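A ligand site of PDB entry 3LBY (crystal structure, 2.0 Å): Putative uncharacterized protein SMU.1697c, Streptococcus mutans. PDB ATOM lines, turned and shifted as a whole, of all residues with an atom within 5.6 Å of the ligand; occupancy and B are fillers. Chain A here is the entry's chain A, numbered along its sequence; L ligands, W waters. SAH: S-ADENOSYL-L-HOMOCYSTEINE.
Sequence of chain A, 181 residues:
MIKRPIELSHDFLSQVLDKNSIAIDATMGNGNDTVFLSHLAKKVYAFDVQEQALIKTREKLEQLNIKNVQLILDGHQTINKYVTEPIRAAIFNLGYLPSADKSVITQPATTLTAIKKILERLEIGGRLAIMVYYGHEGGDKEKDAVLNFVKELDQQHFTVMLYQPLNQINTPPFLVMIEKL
The backbone carbonyl oxygen (O) of Asn 93 sits close to a sulfur (SD) of the ligand, at 3.8 Å. Merely in contact with the ligand: Ala 26 (3.4 Å), Thr 27 (3.7 Å), Gly 29 (3.6 Å), Val 49 (3.6 Å), Gly 75 (3.3 Å), Leu 97 (3.6 Å), Val 104 (3.5 Å), Ile 105 (3.9 Å), Thr 106 (3.6 Å) and Tyr 133 (3.4 Å). Along chain A the residues within 4 Å of the ligand span positions 26 to 133. The nearest printed residue that does not touch the ligand is Phe 47 (4.04 Å).
The side-chain amide oxygen (OD1) of Asn 93 is in hydrogen-bond range of the side-chain hydroxyl (OH) of Tyr 133 (3.3 Å). The side-chain amide oxygen of Gln 107 sits close to the backbone carbonyl oxygen of Ile 105, at 3.4 Å. The backbone NH (N) of Gly 95 lies within hydrogen-bond range of the side-chain hydroxyl (OG1) of Thr 106, 2.9 Å away. OD2 of Asp 48 sits at hydrogen-bond distance from N of Gly 29 (2.9 Å). OD1 of Asp 48 is in hydrogen-bond range of N of Gln 50, 2.9 Å away. The backbone NH (N) of Asp 74 is in hydrogen-bond range of the backbone carbonyl oxygen (O) of Asp 48 (3.0 Å). The backbone NH (N) of Asn 93 sits at hydrogen-bond distance from the side-chain hydroxyl (OG1) of Thr 27. O of Ala 26 sits at hydrogen-bond distance from ND1 of His 76 (2.7 Å).
The backbone carbonyl oxygen of Gly 95 lies within hydrogen-bond range of a nitrogen (N) of the ligand (2.5 Å). O of Leu 94 is in hydrogen-bond range of N of the ligand. N1 of the ligand is in hydrogen-bond range of N of His 76 (2.9 Å). The side-chain amide oxygen (OE1) of Gln 77 sits at hydrogen-bond distance from a nitrogen (N6) of the ligand, at 3.4 Å. An oxygen (O2') of the ligand lies within hydrogen-bond range of the side-chain amide oxygen (OE1) of Gln 50 (2.8 Å). N of the ligand lies within hydrogen-bond range of O of Tyr 96 (2.8 Å). O3' of the ligand lies within hydrogen-bond range of OD2 of Asp 48, at 2.8 Å. ND1 of His 76 lies close to N1 of the ligand (3.3 Å).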
ATOM      1  N   ALA A  26     -14.755 -22.511  21.643  1.00  0.00           N
ATOM      2  CA  ALA A  26     -14.398 -22.049  20.296  1.00  0.00           C
ATOM      3  C   ALA A  26     -15.480 -22.251  19.227  1.00  0.00           C
ATOM      4  O   ALA A  26     -15.371 -21.711  18.125  1.00  0.00           O
ATOM      5  CB  ALA A  26     -13.051 -22.684  19.858  1.00  0.00           C
ATOM      6  N   THR A  27     -16.497 -23.033  19.570  1.00  0.00           N
ATOM      7  CA  THR A  27     -17.582 -23.359  18.645  1.00  0.00           C
ATOM      8  C   THR A  27     -18.913 -23.401  19.392  1.00  0.00           C
ATOM      9  O   THR A  27     -19.473 -24.460  19.673  1.00  0.00           O
ATOM     10  CB  THR A  27     -17.340 -24.726  17.971  1.00  0.00           C
ATOM     11  OG1 THR A  27     -17.022 -25.684  18.976  1.00  0.00           O
ATOM     12  CG2 THR A  27     -16.169 -24.627  16.979  1.00  0.00           C
ATOM     13  N   MET A  28     -19.416 -22.210  19.701  1.00  0.00           N
ATOM     14  CA  MET A  28     -20.600 -22.023  20.530  1.00  0.00           C
ATOM     15  C   MET A  28     -21.786 -22.926  20.163  1.00  0.00           C
ATOM     16  O   MET A  28     -22.396 -23.538  21.031  1.00  0.00           O
ATOM     17  CB  MET A  28     -21.024 -20.560  20.427  1.00  0.00           C
ATOM     18  CG  MET A  28     -22.062 -20.121  21.407  1.00  0.00           C
ATOM     19  SD  MET A  28     -22.614 -18.464  21.008  1.00  0.00           S
ATOM     20  CE  MET A  28     -21.064 -17.571  20.910  1.00  0.00           C
ATOM     21  N   GLY A  29     -22.118 -22.979  18.876  1.00  0.00           N
ATOM     22  CA  GLY A  29     -23.274 -23.736  18.422  1.00  0.00           C
ATOM     23  C   GLY A  29     -24.535 -23.388  19.233  1.00  0.00           C
ATOM     24  O   GLY A  29     -24.837 -22.221  19.464  1.00  0.00           O
ATOM     25  N   PHE A  47     -17.295 -18.395  21.031  1.00  0.00           N
ATOM     26  CA  PHE A  47     -17.187 -17.858  19.667  1.00  0.00           C
ATOM     27  C   PHE A  47     -18.095 -18.596  18.701  1.00  0.00           C
ATOM     28  O   PHE A  47     -18.213 -19.814  18.760  1.00  0.00           O
ATOM     29  CB  PHE A  47     -15.750 -18.054  19.133  1.00  0.00           C
ATOM     30  CG  PHE A  47     -14.721 -17.212  19.815  1.00  0.00           C
ATOM     31  CD1 PHE A  47     -14.261 -16.032  19.236  1.00  0.00           C
ATOM     32  CD2 PHE A  47     -14.167 -17.608  21.032  1.00  0.00           C
ATOM     33  CE1 PHE A  47     -13.297 -15.261  19.862  1.00  0.00           C
ATOM     34  CE2 PHE A  47     -13.204 -16.837  21.658  1.00  0.00           C
ATOM     35  CZ  PHE A  47     -12.767 -15.658  21.082  1.00  0.00           C
ATOM     36  N   ASP A  48     -18.717 -17.851  17.798  1.00  0.00           N
ATOM     37  CA  ASP A  48     -19.389 -18.452  16.641  1.00  0.00           C
ATOM     38  C   ASP A  48     -19.459 -17.452  15.500  1.00  0.00           C
ATOM     39  O   ASP A  48     -19.399 -16.235  15.717  1.00  0.00           O
ATOM     40  CB  ASP A  48     -20.787 -18.964  16.987  1.00  0.00           C
ATOM     41  CG  ASP A  48     -21.197 -20.150  16.130  1.00  0.00           C
ATOM     42  OD1 ASP A  48     -21.360 -20.000  14.896  1.00  0.00           O
ATOM     43  OD2 ASP A  48     -21.332 -21.261  16.678  1.00  0.00           O
ATOM     44  N   VAL A  49     -19.600 -17.969  14.279  1.00  0.00           N
ATOM     45  CA  VAL A  49     -19.788 -17.110  13.116  1.00  0.00           C
ATOM     46  C   VAL A  49     -21.250 -16.997  12.649  1.00  0.00           C
ATOM     47  O   VAL A  49     -21.553 -16.213  11.743  1.00  0.00           O
ATOM     48  CB  VAL A  49     -18.910 -17.550  11.930  1.00  0.00           C
ATOM     49  CG1 VAL A  49     -17.423 -17.511  12.307  1.00  0.00           C
ATOM     50  CG2 VAL A  49     -19.325 -18.935  11.457  1.00  0.00           C
ATOM     51  N   GLN A  50     -22.142 -17.789  13.245  1.00  0.00           N
ATOM     52  CA  GLN A  50     -23.579 -17.734  12.912  1.00  0.00           C
ATOM     53  C   GLN A  50     -24.400 -17.027  13.986  1.00  0.00           C
ATOM     54  O   GLN A  50     -24.352 -17.402  15.159  1.00  0.00           O
ATOM     55  CB  GLN A  50     -24.150 -19.135  12.687  1.00  0.00           C
ATOM     56  CG  GLN A  50     -23.690 -19.860  11.431  1.00  0.00           C
ATOM     57  CD  GLN A  50     -24.337 -21.233  11.259  1.00  0.00           C
ATOM     58  OE1 GLN A  50     -23.716 -22.275  11.526  1.00  0.00           O
ATOM     59  NE2 GLN A  50     -25.597 -21.252  10.832  1.00  0.00           N
ATOM     60  N   ALA A  53     -26.425 -19.115  16.422  1.00  0.00           N
ATOM     61  CA  ALA A  53     -25.734 -19.688  17.572  1.00  0.00           C
ATOM     62  C   ALA A  53     -25.833 -18.767  18.772  1.00  0.00           C
ATOM     63  O   ALA A  53     -26.132 -19.203  19.890  1.00  0.00           O
ATOM     64  CB  ALA A  53     -24.251 -19.964  17.230  1.00  0.00           C
ATOM     65  N   ASP A  74     -17.663 -13.811  15.984  1.00  0.00           N
ATOM     66  CA  ASP A  74     -16.433 -13.698  15.226  1.00  0.00           C
ATOM     67  C   ASP A  74     -15.726 -15.052  15.229  1.00  0.00           C
ATOM     68  O   ASP A  74     -15.981 -15.882  16.103  1.00  0.00           O
ATOM     69  CB  ASP A  74     -15.530 -12.615  15.829  1.00  0.00           C
ATOM     70  CG  ASP A  74     -14.672 -11.919  14.780  1.00  0.00           C
ATOM     71  OD1 ASP A  74     -14.615 -12.397  13.636  1.00  0.00           O
ATOM     72  OD2 ASP A  74     -14.050 -10.883  15.117  1.00  0.00           O
ATOM     73  N   GLY A  75     -14.865 -15.297  14.243  1.00  0.00           N
ATOM     74  CA  GLY A  75     -14.192 -16.583  14.117  1.00  0.00           C
ATOM     75  C   GLY A  75     -13.290 -16.887  15.293  1.00  0.00           C
ATOM     76  O   GLY A  75     -12.642 -15.991  15.832  1.00  0.00           O
ATOM     77  N   HIS A  76     -13.216 -18.157  15.693  1.00  0.00           N
ATOM     78  CA  HIS A  76     -12.298 -18.521  16.783  1.00  0.00           C
ATOM     79  C   HIS A  76     -10.836 -18.187  16.466  1.00  0.00           C
ATOM     80  O   HIS A  76     -10.007 -18.052  17.371  1.00  0.00           O
ATOM     81  CB  HIS A  76     -12.450 -19.996  17.200  1.00  0.00           C
ATOM     82  CG  HIS A  76     -12.638 -20.944  16.065  1.00  0.00           C
ATOM     83  ND1 HIS A  76     -13.584 -21.956  16.093  1.00  0.00           N
ATOM     84  CD2 HIS A  76     -11.988 -21.067  14.875  1.00  0.00           C
ATOM     85  CE1 HIS A  76     -13.514 -22.642  14.959  1.00  0.00           C
ATOM     86  NE2 HIS A  76     -12.561 -22.132  14.213  1.00  0.00           N
ATOM     87  N   GLN A  77     -10.520 -18.021  15.179  1.00  0.00           N
ATOM     88  CA  GLN A  77      -9.167 -17.644  14.781  1.00  0.00           C
ATOM     89  C   GLN A  77      -8.815 -16.220  15.233  1.00  0.00           C
ATOM     90  O   GLN A  77      -7.658 -15.825  15.201  1.00  0.00           O
ATOM     91  CB  GLN A  77      -8.954 -17.808  13.260  1.00  0.00           C
ATOM     92  CG  GLN A  77      -9.665 -16.758  12.381  1.00  0.00           C
ATOM     93  CD  GLN A  77     -11.093 -17.155  12.018  1.00  0.00           C
ATOM     94  OE1 GLN A  77     -11.634 -18.129  12.543  1.00  0.00           O
ATOM     95  NE2 GLN A  77     -11.715 -16.395  11.121  1.00  0.00           N
ATOM     96  N   ASN A  93     -15.887 -28.199  19.083  1.00  0.00           N
ATOM     97  CA  ASN A  93     -16.744 -29.227  18.502  1.00  0.00           C
ATOM     98  C   ASN A  93     -16.853 -28.952  17.009  1.00  0.00           C
ATOM     99  O   ASN A  93     -17.671 -28.126  16.597  1.00  0.00           O
ATOM    100  CB  ASN A  93     -18.137 -29.210  19.113  1.00  0.00           C
ATOM    101  CG  ASN A  93     -18.275 -30.164  20.259  1.00  0.00           C
ATOM    102  OD1 ASN A  93     -18.902 -31.213  20.132  1.00  0.00           O
ATOM    103  ND2 ASN A  93     -17.691 -29.815  21.392  1.00  0.00           N
ATOM    104  N   LEU A  94     -16.039 -29.628  16.208  1.00  0.00           N
ATOM    105  CA  LEU A  94     -15.980 -29.356  14.773  1.00  0.00           C
ATOM    106  C   LEU A  94     -17.178 -29.891  13.968  1.00  0.00           C
ATOM    107  O   LEU A  94     -17.975 -30.679  14.474  1.00  0.00           O
ATOM    108  CB  LEU A  94     -14.662 -29.875  14.193  1.00  0.00           C
ATOM    109  CG  LEU A  94     -13.426 -29.405  14.975  1.00  0.00           C
ATOM    110  CD1 LEU A  94     -12.162 -30.042  14.411  1.00  0.00           C
ATOM    111  CD2 LEU A  94     -13.341 -27.877  14.979  1.00  0.00           C
ATOM    112  N   GLY A  95     -17.310 -29.423  12.729  1.00  0.00           N
ATOM    113  CA  GLY A  95     -18.309 -29.935  11.788  1.00  0.00           C
ATOM    114  C   GLY A  95     -19.804 -29.683  11.969  1.00  0.00           C
ATOM    115  O   GLY A  95     -20.547 -30.627  12.254  1.00  0.00           O
ATOM    116  N   TYR A  96     -20.250 -28.437  11.801  1.00  0.00           N
ATOM    117  CA  TYR A  96     -21.685 -28.071  11.642  1.00  0.00           C
ATOM    118  C   TYR A  96     -22.735 -28.470  12.705  1.00  0.00           C
ATOM    119  O   TYR A  96     -22.704 -29.555  13.268  1.00  0.00           O
ATOM    120  CB  TYR A  96     -22.187 -28.451  10.238  1.00  0.00           C
ATOM    121  CG  TYR A  96     -22.853 -29.808  10.121  1.00  0.00           C
ATOM    122  CD1 TYR A  96     -24.153 -30.010  10.564  1.00  0.00           C
ATOM    123  CD2 TYR A  96     -22.184 -30.892   9.552  1.00  0.00           C
ATOM    124  CE1 TYR A  96     -24.767 -31.252  10.453  1.00  0.00           C
ATOM    125  CE2 TYR A  96     -22.787 -32.130   9.433  1.00  0.00           C
ATOM    126  CZ  TYR A  96     -24.078 -32.310   9.883  1.00  0.00           C
ATOM    127  OH  TYR A  96     -24.692 -33.535   9.778  1.00  0.00           O
ATOM    128  N   LEU A  97     -23.693 -27.561  12.921  1.00  0.00           N
ATOM    129  CA  LEU A  97     -24.832 -27.839  13.800  1.00  0.00           C
ATOM    130  C   LEU A  97     -26.129 -27.929  12.999  1.00  0.00           C
ATOM    131  O   LEU A  97     -26.248 -27.338  11.936  1.00  0.00           O
ATOM    132  CB  LEU A  97     -24.973 -26.750  14.872  1.00  0.00           C
ATOM    133  CG  LEU A  97     -25.815 -25.524  14.511  1.00  0.00           C
ATOM    134  CD1 LEU A  97     -26.190 -24.725  15.752  1.00  0.00           C
ATOM    135  CD2 LEU A  97     -25.095 -24.643  13.494  1.00  0.00           C
ATOM    136  N   PRO A  98     -27.102 -28.698  13.517  1.00  0.00           N
ATOM    137  CA  PRO A  98     -28.441 -28.834  12.911  1.00  0.00           C
ATOM    138  C   PRO A  98     -29.140 -27.494  12.642  1.00  0.00           C
ATOM    139  O   PRO A  98     -30.042 -27.115  13.379  1.00  0.00           O
ATOM    140  CB  PRO A  98     -29.212 -29.632  13.954  1.00  0.00           C
ATOM    141  CG  PRO A  98     -28.170 -30.468  14.619  1.00  0.00           C
ATOM    142  CD  PRO A  98     -26.930 -29.601  14.665  1.00  0.00           C
ATOM    143  N   VAL A 104     -21.872 -23.685   6.690  1.00  0.00           N
ATOM    144  CA  VAL A 104     -21.188 -23.062   7.822  1.00  0.00           C
ATOM    145  C   VAL A 104     -20.472 -24.102   8.688  1.00  0.00           C
ATOM    146  O   VAL A 104     -20.574 -24.091   9.919  1.00  0.00           O
ATOM    147  CB  VAL A 104     -22.113 -22.212   8.700  1.00  0.00           C
ATOM    148  CG1 VAL A 104     -21.263 -21.292   9.562  1.00  0.00           C
ATOM    149  CG2 VAL A 104     -23.076 -21.398   7.838  1.00  0.00           C
ATOM    150  N   ILE A 105     -19.745 -24.993   8.040  1.00  0.00           N
ATOM    151  CA  ILE A 105     -18.920 -25.937   8.773  1.00  0.00           C
ATOM    152  C   ILE A 105     -17.607 -25.264   9.162  1.00  0.00           C
ATOM    153  O   ILE A 105     -17.190 -24.275   8.547  1.00  0.00           O
ATOM    154  CB  ILE A 105     -18.624 -27.197   7.956  1.00  0.00           C
ATOM    155  CG1 ILE A 105     -17.987 -26.831   6.621  1.00  0.00           C
ATOM    156  CG2 ILE A 105     -19.911 -28.002   7.734  1.00  0.00           C
ATOM    157  CD1 ILE A 105     -17.347 -28.020   5.909  1.00  0.00           C
ATOM    158  N   THR A 106     -16.963 -25.819  10.181  1.00  0.00           N
ATOM    159  CA  THR A 106     -15.629 -25.381  10.567  1.00  0.00           C
ATOM    160  C   THR A 106     -14.684 -25.805   9.454  1.00  0.00           C
ATOM    161  O   THR A 106     -14.929 -26.806   8.774  1.00  0.00           O
ATOM    162  CB  THR A 106     -15.199 -26.004  11.907  1.00  0.00           C
ATOM    163  OG1 THR A 106     -15.358 -27.438  11.850  1.00  0.00           O
ATOM    164  CG2 THR A 106     -16.073 -25.458  13.042  1.00  0.00           C
ATOM    165  N   GLN A 107     -13.586 -25.067   9.303  1.00  0.00           N
ATOM    166  CA  GLN A 107     -12.691 -25.249   8.168  1.00  0.00           C
ATOM    167  C   GLN A 107     -11.251 -25.417   8.633  1.00  0.00           C
ATOM    168  O   GLN A 107     -10.862 -24.847   9.660  1.00  0.00           O
ATOM    169  CB  GLN A 107     -12.794 -24.033   7.238  1.00  0.00           C
ATOM    170  CG  GLN A 107     -12.962 -24.387   5.786  1.00  0.00           C
ATOM    171  CD  GLN A 107     -14.280 -25.071   5.509  1.00  0.00           C
ATOM    172  OE1 GLN A 107     -15.349 -24.485   5.693  1.00  0.00           O
ATOM    173  NE2 GLN A 107     -14.221 -26.327   5.059  1.00  0.00           N
ATOM    174  N   THR A 110      -8.856 -22.122   9.504  1.00  0.00           N
ATOM    175  CA  THR A 110      -9.372 -21.351  10.641  1.00  0.00           C
ATOM    176  C   THR A 110      -9.314 -22.171  11.923  1.00  0.00           C
ATOM    177  O   THR A 110      -8.979 -21.655  12.991  1.00  0.00           O
ATOM    178  CB  THR A 110     -10.800 -20.823  10.382  1.00  0.00           C
ATOM    179  OG1 THR A 110     -11.606 -21.852   9.786  1.00  0.00           O
ATOM    180  CG2 THR A 110     -10.760 -19.605   9.477  1.00  0.00           C
ATOM    181  N   TYR A 133     -15.846 -34.210  14.212  1.00  0.00           N
ATOM    182  CA  TYR A 133     -16.938 -34.813  13.441  1.00  0.00           C
ATOM    183  C   TYR A 133     -16.551 -34.798  11.970  1.00  0.00           C
ATOM    184  O   TYR A 133     -16.075 -33.790  11.468  1.00  0.00           O
ATOM    185  CB  TYR A 133     -18.249 -34.026  13.617  1.00  0.00           C
ATOM    186  CG  TYR A 133     -18.772 -34.031  15.028  1.00  0.00           C
ATOM    187  CD1 TYR A 133     -19.856 -34.808  15.392  1.00  0.00           C
ATOM    188  CD2 TYR A 133     -18.167 -33.274  16.019  1.00  0.00           C
ATOM    189  CE1 TYR A 133     -20.328 -34.828  16.682  1.00  0.00           C
ATOM    190  CE2 TYR A 133     -18.620 -33.284  17.302  1.00  0.00           C
ATOM    191  CZ  TYR A 133     -19.703 -34.059  17.643  1.00  0.00           C
ATOM    192  OH  TYR A 133     -20.143 -34.056  18.937  1.00  0.00           O
HETATM  193  N   SAH L   1     -20.916 -31.314  14.580  1.00  0.00           N
HETATM  194  CA  SAH L   1     -21.003 -31.144  16.053  1.00  0.00           C
HETATM  195  CB  SAH L   1     -20.784 -29.680  16.449  1.00  0.00           C
HETATM  196  CG  SAH L   1     -20.895 -28.660  15.321  1.00  0.00           C
HETATM  197  SD  SAH L   1     -21.240 -27.014  15.990  1.00  0.00           S
HETATM  198  C   SAH L   1     -22.308 -31.687  16.625  1.00  0.00           C
HETATM  199  O   SAH L   1     -23.038 -32.410  15.944  1.00  0.00           O
HETATM  200  OXT SAH L   1     -22.652 -31.447  17.775  1.00  0.00           O
HETATM  201  C5' SAH L   1     -19.929 -26.203  15.015  1.00  0.00           C
HETATM  202  C4' SAH L   1     -20.100 -24.688  15.069  1.00  0.00           C
HETATM  203  O4' SAH L   1     -18.918 -24.051  14.637  1.00  0.00           O
HETATM  204  C3' SAH L   1     -21.235 -24.117  14.208  1.00  0.00           C
HETATM  205  O3' SAH L   1     -22.101 -23.358  15.034  1.00  0.00           O
HETATM  206  C2' SAH L   1     -20.528 -23.161  13.252  1.00  0.00           C
HETATM  207  O2' SAH L   1     -21.297 -22.015  12.972  1.00  0.00           O
HETATM  208  C1' SAH L   1     -19.298 -22.809  14.065  1.00  0.00           C
HETATM  209  N9  SAH L   1     -18.186 -22.269  13.277  1.00  0.00           N
HETATM  210  C8  SAH L   1     -17.872 -22.524  11.958  1.00  0.00           C
HETATM  211  N7  SAH L   1     -16.752 -21.826  11.673  1.00  0.00           N
HETATM  212  C5  SAH L   1     -16.349 -21.135  12.768  1.00  0.00           C
HETATM  213  C6  SAH L   1     -15.284 -20.283  13.011  1.00  0.00           C
HETATM  214  N6  SAH L   1     -14.393 -19.994  12.067  1.00  0.00           N
HETATM  215  N1  SAH L   1     -15.142 -19.741  14.280  1.00  0.00           N
HETATM  216  C2  SAH L   1     -16.046 -20.022  15.282  1.00  0.00           C
HETATM  217  N3  SAH L   1     -17.105 -20.879  15.021  1.00  0.00           N
HETATM  218  C4  SAH L   1     -17.251 -21.421  13.784  1.00  0.00           C
HETATM  219  O   HOH W   1     -23.100 -33.889  13.036  1.00  0.00           O
